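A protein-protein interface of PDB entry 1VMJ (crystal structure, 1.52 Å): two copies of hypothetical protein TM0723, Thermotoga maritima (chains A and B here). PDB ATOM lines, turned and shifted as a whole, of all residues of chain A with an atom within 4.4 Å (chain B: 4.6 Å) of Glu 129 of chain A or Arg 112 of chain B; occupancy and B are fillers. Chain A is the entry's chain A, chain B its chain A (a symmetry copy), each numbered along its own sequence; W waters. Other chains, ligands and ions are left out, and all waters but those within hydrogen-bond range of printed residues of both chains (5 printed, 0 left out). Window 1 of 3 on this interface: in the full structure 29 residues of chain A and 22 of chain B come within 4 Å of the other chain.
The guanidinium group (NH2) of Arg 107 of chain B lies within hydrogen-bond range of the backbone carbonyl oxygen (O) of Ile 64 of chain A (2.8 Å).
O of Ile 58 of chain B is in hydrogen-bond range of ND2 of Asn 65 of chain A, at 3.4 Å.
The guanidinium group of Arg 112 of chain B is in hydrogen-bond range of the backbone carbonyl oxygen of Val 115 of chain A, at 2.9 Å.
N of Val 115 of chain A lies within hydrogen-bond range of OE2 of Glu 113 of chain B (3.0 Å).
The guanidinium group of Arg 112 of chain B is in salt-bridge range of the side-chain carboxylate of Glu 129 of chain A, at 2.9 Å.
N of Asn 65 of chain A lies within hydrogen-bond range of O of Gln 130 of chain A.
The guanidinium group (NH2) of Arg 112 of chain B sits close to the side-chain amide nitrogen (ND2) of Asn 54 of chain B.
O of Arg 112 of chain B is in hydrogen-bond range of N of Ala 55 of chain B, at 3.0 Å.
The backbone carbonyl oxygen of Arg 107 of chain B is in hydrogen-bond range of the side-chain hydroxyl of Ser 61 of chain B (3.1 Å).
The backbone carbonyl oxygen of Arg 112 of chain B lies within hydrogen-bond range of the backbone NH of Val 62 of chain B (3.5 Å).
The guanidinium group (NH1) of Arg 112 of chain B lies within salt-bridge range of the side-chain carboxylate (OE1) of Glu 113 of chain B, 2.8 Å away.
Among the printed residues, pairs that only touch across the chains: Ile 64 of chain A with Arg 112 of chain B, Asn 65 of chain A with Arg 107 of chain B, Leu 125 of chain A with Met 56 of chain B, Gly 126 of chain A with Met 56 of chain B, Trp 128 of chain A with Ile 58 of chain B, Glu 129 of chain A with Ala 55 of chain B, Glu 129 of chain A with Met 56 of chain B and Glu 129 of chain A with Ile 58 of chain B.
Of the printed residues of chain B, Ile 64 of chain A touches Arg 107 and Arg 112.
Ile 116 of chain A touches none of the printed residues of chain B.
Pro 127 of chain A touches none of the printed residues of chain B.
Of the printed residues of chain B, Trp 128 of chain A touches Ile 58.
Glu 129 of chain A touches four residues of chain B.
Of the printed residues of chain A, Ala 55 of chain B touches Glu 129.
Of the printed residues of chain A, Arg 107 of chain B touches Ile 64 and Asn 65.
Printed residues of chain A within 4 Å of Glu 113 of chain B: Val 115 (3.0 Å).
The nearest residue of chain B that does not touch Glu 129 of chain A is Asn 54 of chain B (4.2 Å).
The nearest residue of chain A that does not touch Arg 112 of chain B is Ile 116 of chain A (4.2 Å).
Hydrophobic or aromatic side chains of chain A within 4 Å of the printed part of chain B: Ile 64, Val 115 and Trp 128.
Along chain A the printed residues that touch a printed residue of chain B span positions 64 to 129.
Of the 11 printed residues of chain B, 6 touch a printed residue of chain A.
Hydrophobic or aromatic side chains of chain B that line the printed part of chain A: Met 56 and Ile 58.
Among the printed residues, Asp or Glu carboxylates within 4 Å of a Lys or Arg side-chain nitrogen of the other chain: Glu 129 of chain A with Arg 112 of chain B (2.9 Å).
No position is printed for both chains.
Water W5 lies within hydrogen-bond range of OE2 of Glu 129 of chain A (2.6 Å), O of Ala 55 of chain B (2.8 Å), NH2 of Arg 107 of chain B (2.9 Å) and NE of Arg 112 of chain B (3.3 Å).
Water W4 lies within hydrogen-bond range of OE1 of Glu 129 of chain A (2.7 Å), O of Asp 124 of chain A (2.7 Å) and ND2 of Asn 54 of chain B (2.8 Å).
Water W1 bridges the backbone carbonyl oxygen (O) of Met 56 of chain B and the backbone NH (N) of Trp 128 of chain A.
Water W2 lies within hydrogen-bond range of OD1 of Asn 54 of chain B (2.8 Å), NH2 of Arg 112 of chain B (3.1 Å) and O of Asp 124 of chain A (3.4 Å).
Water W3 lies within hydrogen-bond range of ND2 of Asn 65 of chain A (2.9 Å), NE of Arg 107 of chain B (3.1 Å) and O of Ile 64 of chain A (3.3 Å).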
ATOM      1  N   ILE A  64      -2.566  25.125  -5.958  1.00  0.00           N
ATOM      2  CA  ILE A  64      -1.196  25.527  -6.222  1.00  0.00           C
ATOM      3  C   ILE A  64      -1.133  26.381  -7.477  1.00  0.00           C
ATOM      4  O   ILE A  64      -1.618  25.979  -8.543  1.00  0.00           O
ATOM      5  CB  ILE A  64      -0.251  24.323  -6.351  1.00  0.00           C
ATOM      6  CG1 ILE A  64       0.037  23.763  -4.947  1.00  0.00           C
ATOM      7  CG2 ILE A  64       1.060  24.713  -7.003  1.00  0.00           C
ATOM      8  CD1 ILE A  64       0.592  22.386  -4.890  1.00  0.00           C
ATOM      9  N   ASN A  65      -0.512  27.556  -7.365  1.00  0.00           N
ATOM     10  CA  ASN A  65      -0.238  28.354  -8.547  1.00  0.00           C
ATOM     11  C   ASN A  65       0.779  29.432  -8.212  1.00  0.00           C
ATOM     12  O   ASN A  65       1.499  29.284  -7.265  1.00  0.00           O
ATOM     13  CB  ASN A  65      -1.541  28.882  -9.181  1.00  0.00           C
ATOM     14  CG  ASN A  65      -1.447  28.892 -10.705  1.00  0.00           C
ATOM     15  OD1 ASN A  65      -0.723  29.722 -11.264  1.00  0.00           O
ATOM     16  ND2 ASN A  65      -2.045  27.891 -11.365  1.00  0.00           N
ATOM     17  N   VAL A 115      -2.499  17.406  -3.345  1.00  0.00           N
ATOM     18  CA  VAL A 115      -1.725  16.314  -2.807  1.00  0.00           C
ATOM     19  C   VAL A 115      -0.301  16.520  -3.298  1.00  0.00           C
ATOM     20  O   VAL A 115      -0.073  16.732  -4.491  1.00  0.00           O
ATOM     21  CB  VAL A 115      -2.264  14.946  -3.256  1.00  0.00           C
ATOM     22  CG1 VAL A 115      -1.398  13.831  -2.692  1.00  0.00           C
ATOM     23  CG2 VAL A 115      -3.719  14.790  -2.813  1.00  0.00           C
ATOM     24  N   ILE A 116       0.639  16.511  -2.363  1.00  0.00           N
ATOM     25  CA  ILE A 116       2.007  16.878  -2.610  1.00  0.00           C
ATOM     26  C   ILE A 116       2.941  15.791  -2.121  1.00  0.00           C
ATOM     27  O   ILE A 116       2.777  15.276  -1.000  1.00  0.00           O
ATOM     28  CB  ILE A 116       2.350  18.215  -1.892  1.00  0.00           C
ATOM     29  CG1 ILE A 116       1.416  19.341  -2.324  1.00  0.00           C
ATOM     30  CG2 ILE A 116       3.801  18.586  -2.132  1.00  0.00           C
ATOM     31  CD1 ILE A 116       1.560  20.545  -1.523  1.00  0.00           C
ATOM     32  N   ASP A 124       7.968  18.214  -2.453  1.00  0.00           N
ATOM     33  CA  ASP A 124       8.674  17.973  -3.704  1.00  0.00           C
ATOM     34  C   ASP A 124       8.003  18.824  -4.780  1.00  0.00           C
ATOM     35  O   ASP A 124       7.060  18.378  -5.439  1.00  0.00           O
ATOM     36  CB  ASP A 124       8.605  16.475  -3.977  1.00  0.00           C
ATOM     37  CG  ASP A 124       9.630  15.982  -4.926  1.00  0.00           C
ATOM     38  OD1 ASP A 124      10.281  16.784  -5.641  1.00  0.00           O
ATOM     39  OD2 ASP A 124       9.763  14.746  -4.984  1.00  0.00           O
ATOM     40  N   LEU A 125       8.448  20.070  -4.889  1.00  0.00           N
ATOM     41  CA  LEU A 125       7.766  21.092  -5.675  1.00  0.00           C
ATOM     42  C   LEU A 125       8.643  21.581  -6.811  1.00  0.00           C
ATOM     43  O   LEU A 125       9.893  21.588  -6.705  1.00  0.00           O
ATOM     44  CB  LEU A 125       7.409  22.301  -4.810  1.00  0.00           C
ATOM     45  CG  LEU A 125       6.447  22.047  -3.650  1.00  0.00           C
ATOM     46  CD1 LEU A 125       6.213  23.298  -2.832  1.00  0.00           C
ATOM     47  CD2 LEU A 125       5.177  21.463  -4.138  1.00  0.00           C
ATOM     48  N   GLY A 126       7.978  22.035  -7.866  1.00  0.00           N
ATOM     49  CA  GLY A 126       8.639  22.703  -8.967  1.00  0.00           C
ATOM     50  C   GLY A 126       8.990  24.113  -8.573  1.00  0.00           C
ATOM     51  O   GLY A 126       8.666  24.552  -7.479  1.00  0.00           O
ATOM     52  N   PRO A 127       9.648  24.835  -9.490  1.00  0.00           N
ATOM     53  CA  PRO A 127      10.278  26.098  -9.157  1.00  0.00           C
ATOM     54  C   PRO A 127       9.328  27.209  -8.719  1.00  0.00           C
ATOM     55  O   PRO A 127       9.725  28.069  -7.942  1.00  0.00           O
ATOM     56  CB  PRO A 127      10.978  26.484 -10.462  1.00  0.00           C
ATOM     57  CG  PRO A 127      10.244  25.774 -11.529  1.00  0.00           C
ATOM     58  CD  PRO A 127       9.847  24.467 -10.905  1.00  0.00           C
ATOM     59  N   TRP A 128       8.097  27.191  -9.210  1.00  0.00           N
ATOM     60  CA  TRP A 128       7.163  28.280  -8.975  1.00  0.00           C
ATOM     61  C   TRP A 128       5.911  27.861  -8.249  1.00  0.00           C
ATOM     62  O   TRP A 128       4.994  28.661  -8.102  1.00  0.00           O
ATOM     63  CB  TRP A 128       6.852  29.006 -10.281  1.00  0.00           C
ATOM     64  CG  TRP A 128       8.102  29.489 -10.933  1.00  0.00           C
ATOM     65  CD1 TRP A 128       8.624  29.056 -12.101  1.00  0.00           C
ATOM     66  CD2 TRP A 128       9.031  30.431 -10.393  1.00  0.00           C
ATOM     67  NE1 TRP A 128       9.824  29.698 -12.347  1.00  0.00           N
ATOM     68  CE2 TRP A 128      10.092  30.545 -11.307  1.00  0.00           C
ATOM     69  CE3 TRP A 128       9.067  31.194  -9.219  1.00  0.00           C
ATOM     70  CZ2 TRP A 128      11.178  31.398 -11.091  1.00  0.00           C
ATOM     71  CZ3 TRP A 128      10.143  32.044  -9.002  1.00  0.00           C
ATOM     72  CH2 TRP A 128      11.182  32.139  -9.937  1.00  0.00           C
ATOM     73  N   GLU A 129       5.868  26.604  -7.804  1.00  0.00           N
ATOM     74  CA  GLU A 129       4.710  26.114  -7.072  1.00  0.00           C
ATOM     75  C   GLU A 129       4.603  26.750  -5.701  1.00  0.00           C
ATOM     76  O   GLU A 129       5.520  26.656  -4.887  1.00  0.00           O
ATOM     77  CB  GLU A 129       4.736  24.598  -6.910  1.00  0.00           C
ATOM     78  CG  GLU A 129       4.596  23.824  -8.197  1.00  0.00           C
ATOM     79  CD  GLU A 129       4.342  22.352  -7.952  1.00  0.00           C
ATOM     80  OE1 GLU A 129       5.326  21.610  -7.769  1.00  0.00           O
ATOM     81  OE2 GLU A 129       3.163  21.934  -7.904  1.00  0.00           O
ATOM     82  N   GLN A 130       3.471  27.401  -5.463  1.00  0.00           N
ATOM     83  CA  GLN A 130       3.131  27.900  -4.142  1.00  0.00           C
ATOM     84  C   GLN A 130       1.725  27.457  -3.796  1.00  0.00           C
ATOM     85  O   GLN A 130       0.860  27.405  -4.658  1.00  0.00           O
ATOM     86  CB  GLN A 130       3.218  29.418  -4.102  1.00  0.00           C
ATOM     87  CG  GLN A 130       4.614  30.000  -4.266  1.00  0.00           C
ATOM     88  CD  GLN A 130       5.473  29.865  -3.036  1.00  0.00           C
ATOM     89  OE1 GLN A 130       5.233  30.511  -2.030  1.00  0.00           O
ATOM     90  NE2 GLN A 130       6.441  28.977  -3.096  1.00  0.00           N
ATOM     91  N   CYS B  53       0.552  11.733  -9.491  1.00  0.00           N
ATOM     92  CA  CYS B  53       1.220  12.258 -10.637  1.00  0.00           C
ATOM     93  C   CYS B  53       0.746  13.684 -10.860  1.00  0.00           C
ATOM     94  O   CYS B  53      -0.452  13.918 -11.101  1.00  0.00           O
ATOM     95  CB  CYS B  53       0.913  11.397 -11.854  1.00  0.00           C
ATOM     96  SG  CYS B  53       1.771  11.953 -13.339  1.00  0.00           S
ATOM     97  N   ASN B  54       1.686  14.627 -10.812  1.00  0.00           N
ATOM     98  CA  ASN B  54       1.345  16.032 -10.906  1.00  0.00           C
ATOM     99  C   ASN B  54       2.275  16.812 -11.803  1.00  0.00           C
ATOM    100  O   ASN B  54       3.439  16.493 -11.931  1.00  0.00           O
ATOM    101  CB  ASN B  54       1.241  16.678  -9.524  1.00  0.00           C
ATOM    102  CG  ASN B  54       2.590  16.836  -8.825  1.00  0.00           C
ATOM    103  OD1 ASN B  54       2.985  15.974  -8.035  1.00  0.00           O
ATOM    104  ND2 ASN B  54       3.299  17.956  -9.082  1.00  0.00           N
ATOM    105  N   ALA B  55       1.715  17.864 -12.414  1.00  0.00           N
ATOM    106  CA  ALA B  55       2.514  18.847 -13.122  1.00  0.00           C
ATOM    107  C   ALA B  55       3.307  19.632 -12.079  1.00  0.00           C
ATOM    108  O   ALA B  55       2.731  20.128 -11.120  1.00  0.00           O
ATOM    109  CB  ALA B  55       1.623  19.746 -13.904  1.00  0.00           C
ATOM    110  N   MET B  56       4.615  19.760 -12.294  1.00  0.00           N
ATOM    111  CA  MET B  56       5.474  20.529 -11.398  1.00  0.00           C
ATOM    112  C   MET B  56       5.508  21.994 -11.789  1.00  0.00           C
ATOM    113  O   MET B  56       6.077  22.812 -11.080  1.00  0.00           O
ATOM    114  CB  MET B  56       6.879  19.966 -11.400  1.00  0.00           C
ATOM    115  CG  MET B  56       6.919  18.531 -10.971  1.00  0.00           C
ATOM    116  SD  MET B  56       8.593  17.887 -10.721  1.00  0.00           S
ATOM    117  CE  MET B  56       8.983  18.460  -9.080  1.00  0.00           C
ATOM    118  N   ILE B  58       3.173  25.417 -13.133  1.00  0.00           N
ATOM    119  CA  ILE B  58       1.870  25.977 -12.786  1.00  0.00           C
ATOM    120  C   ILE B  58       1.076  26.429 -14.008  1.00  0.00           C
ATOM    121  O   ILE B  58       0.031  27.084 -13.871  1.00  0.00           O
ATOM    122  CB  ILE B  58       2.033  27.096 -11.711  1.00  0.00           C
ATOM    123  CG1 ILE B  58       2.956  28.202 -12.225  1.00  0.00           C
ATOM    124  CG2 ILE B  58       2.570  26.509 -10.402  1.00  0.00           C
ATOM    125  CD1 ILE B  58       3.077  29.392 -11.305  1.00  0.00           C
ATOM    126  N   SER B  61      -0.924  20.630 -16.723  1.00  0.00           N
ATOM    127  CA  SER B  61      -1.826  19.729 -16.000  1.00  0.00           C
ATOM    128  C   SER B  61      -1.429  18.290 -16.132  1.00  0.00           C
ATOM    129  O   SER B  61      -0.805  17.908 -17.106  1.00  0.00           O
ATOM    130  CB  SER B  61      -3.249  19.837 -16.571  1.00  0.00           C
ATOM    131  OG  SER B  61      -3.790  21.117 -16.322  1.00  0.00           O
ATOM    132  N   VAL B  62      -1.853  17.487 -15.159  1.00  0.00           N
ATOM    133  CA  VAL B  62      -1.969  16.040 -15.327  1.00  0.00           C
ATOM    134  C   VAL B  62      -3.422  15.661 -15.030  1.00  0.00           C
ATOM    135  O   VAL B  62      -3.992  16.081 -14.035  1.00  0.00           O
ATOM    136  CB  VAL B  62      -1.023  15.271 -14.438  1.00  0.00           C
ATOM    137  CG1 VAL B  62      -1.272  13.788 -14.549  1.00  0.00           C
ATOM    138  CG2 VAL B  62       0.419  15.577 -14.809  1.00  0.00           C
ATOM    139  N   ARG B 107      -4.864  25.318 -16.958  1.00  0.00           N
ATOM    140  CA  ARG B 107      -4.412  24.196 -16.121  1.00  0.00           C
ATOM    141  C   ARG B 107      -5.335  24.046 -14.934  1.00  0.00           C
ATOM    142  O   ARG B 107      -5.550  22.921 -14.470  1.00  0.00           O
ATOM    143  CB  ARG B 107      -2.937  24.341 -15.714  1.00  0.00           C
ATOM    144  CG  ARG B 107      -2.627  24.840 -14.293  1.00  0.00           C
ATOM    145  CD  ARG B 107      -2.869  23.818 -13.220  1.00  0.00           C
ATOM    146  NE  ARG B 107      -2.244  24.143 -11.935  1.00  0.00           N
ATOM    147  CZ  ARG B 107      -1.040  23.755 -11.566  1.00  0.00           C
ATOM    148  NH1 ARG B 107      -0.279  23.014 -12.351  1.00  0.00           N
ATOM    149  NH2 ARG B 107      -0.577  24.089 -10.374  1.00  0.00           N
ATOM    150  N   GLY B 111      -6.847  20.565 -14.057  1.00  0.00           N
ATOM    151  CA  GLY B 111      -6.291  20.086 -12.812  1.00  0.00           C
ATOM    152  C   GLY B 111      -4.786  19.932 -12.810  1.00  0.00           C
ATOM    153  O   GLY B 111      -4.143  19.686 -13.820  1.00  0.00           O
ATOM    154  N   ARG B 112      -4.224  20.004 -11.621  1.00  0.00           N
ATOM    155  CA  ARG B 112      -2.805  19.819 -11.423  1.00  0.00           C
ATOM    156  C   ARG B 112      -2.327  18.371 -11.404  1.00  0.00           C
ATOM    157  O   ARG B 112      -1.218  18.085 -11.818  1.00  0.00           O
ATOM    158  CB  ARG B 112      -2.418  20.484 -10.091  1.00  0.00           C
ATOM    159  CG  ARG B 112      -1.007  20.154  -9.612  1.00  0.00           C
ATOM    160  CD  ARG B 112      -0.717  20.828  -8.297  1.00  0.00           C
ATOM    161  NE  ARG B 112       0.600  20.537  -7.783  1.00  0.00           N
ATOM    162  CZ  ARG B 112       0.872  19.540  -6.957  1.00  0.00           C
ATOM    163  NH1 ARG B 112      -0.076  18.713  -6.559  1.00  0.00           N
ATOM    164  NH2 ARG B 112       2.098  19.416  -6.471  1.00  0.00           N
ATOM    165  N   GLU B 113      -3.150  17.486 -10.842  1.00  0.00           N
ATOM    166  CA  GLU B 113      -2.691  16.177 -10.412  1.00  0.00           C
ATOM    167  C   GLU B 113      -3.775  15.125 -10.604  1.00  0.00           C
ATOM    168  O   GLU B 113      -4.960  15.442 -10.736  1.00  0.00           O
ATOM    169  CB  GLU B 113      -2.223  16.213  -8.951  1.00  0.00           C
ATOM    170  CG  GLU B 113      -3.386  16.238  -7.974  1.00  0.00           C
ATOM    171  CD  GLU B 113      -3.393  17.290  -6.830  1.00  0.00           C
ATOM    172  OE1 GLU B 113      -2.804  18.394  -6.883  1.00  0.00           O
ATOM    173  OE2 GLU B 113      -4.095  16.990  -5.834  1.00  0.00           O
HETATM  174  O   HOH W   1       6.768  25.541 -11.103  1.00  0.00           O
HETATM  175  O   HOH W   2       3.918  17.006  -5.580  1.00  0.00           O
HETATM  176  O   HOH W   3      -4.176  26.097 -10.580  1.00  0.00           O
HETATM  177  O   HOH W   4       5.418  18.969  -7.486  1.00  0.00           O
HETATM  178  O   HOH W   5       1.846  22.573 -10.087  1.00  0.00           O
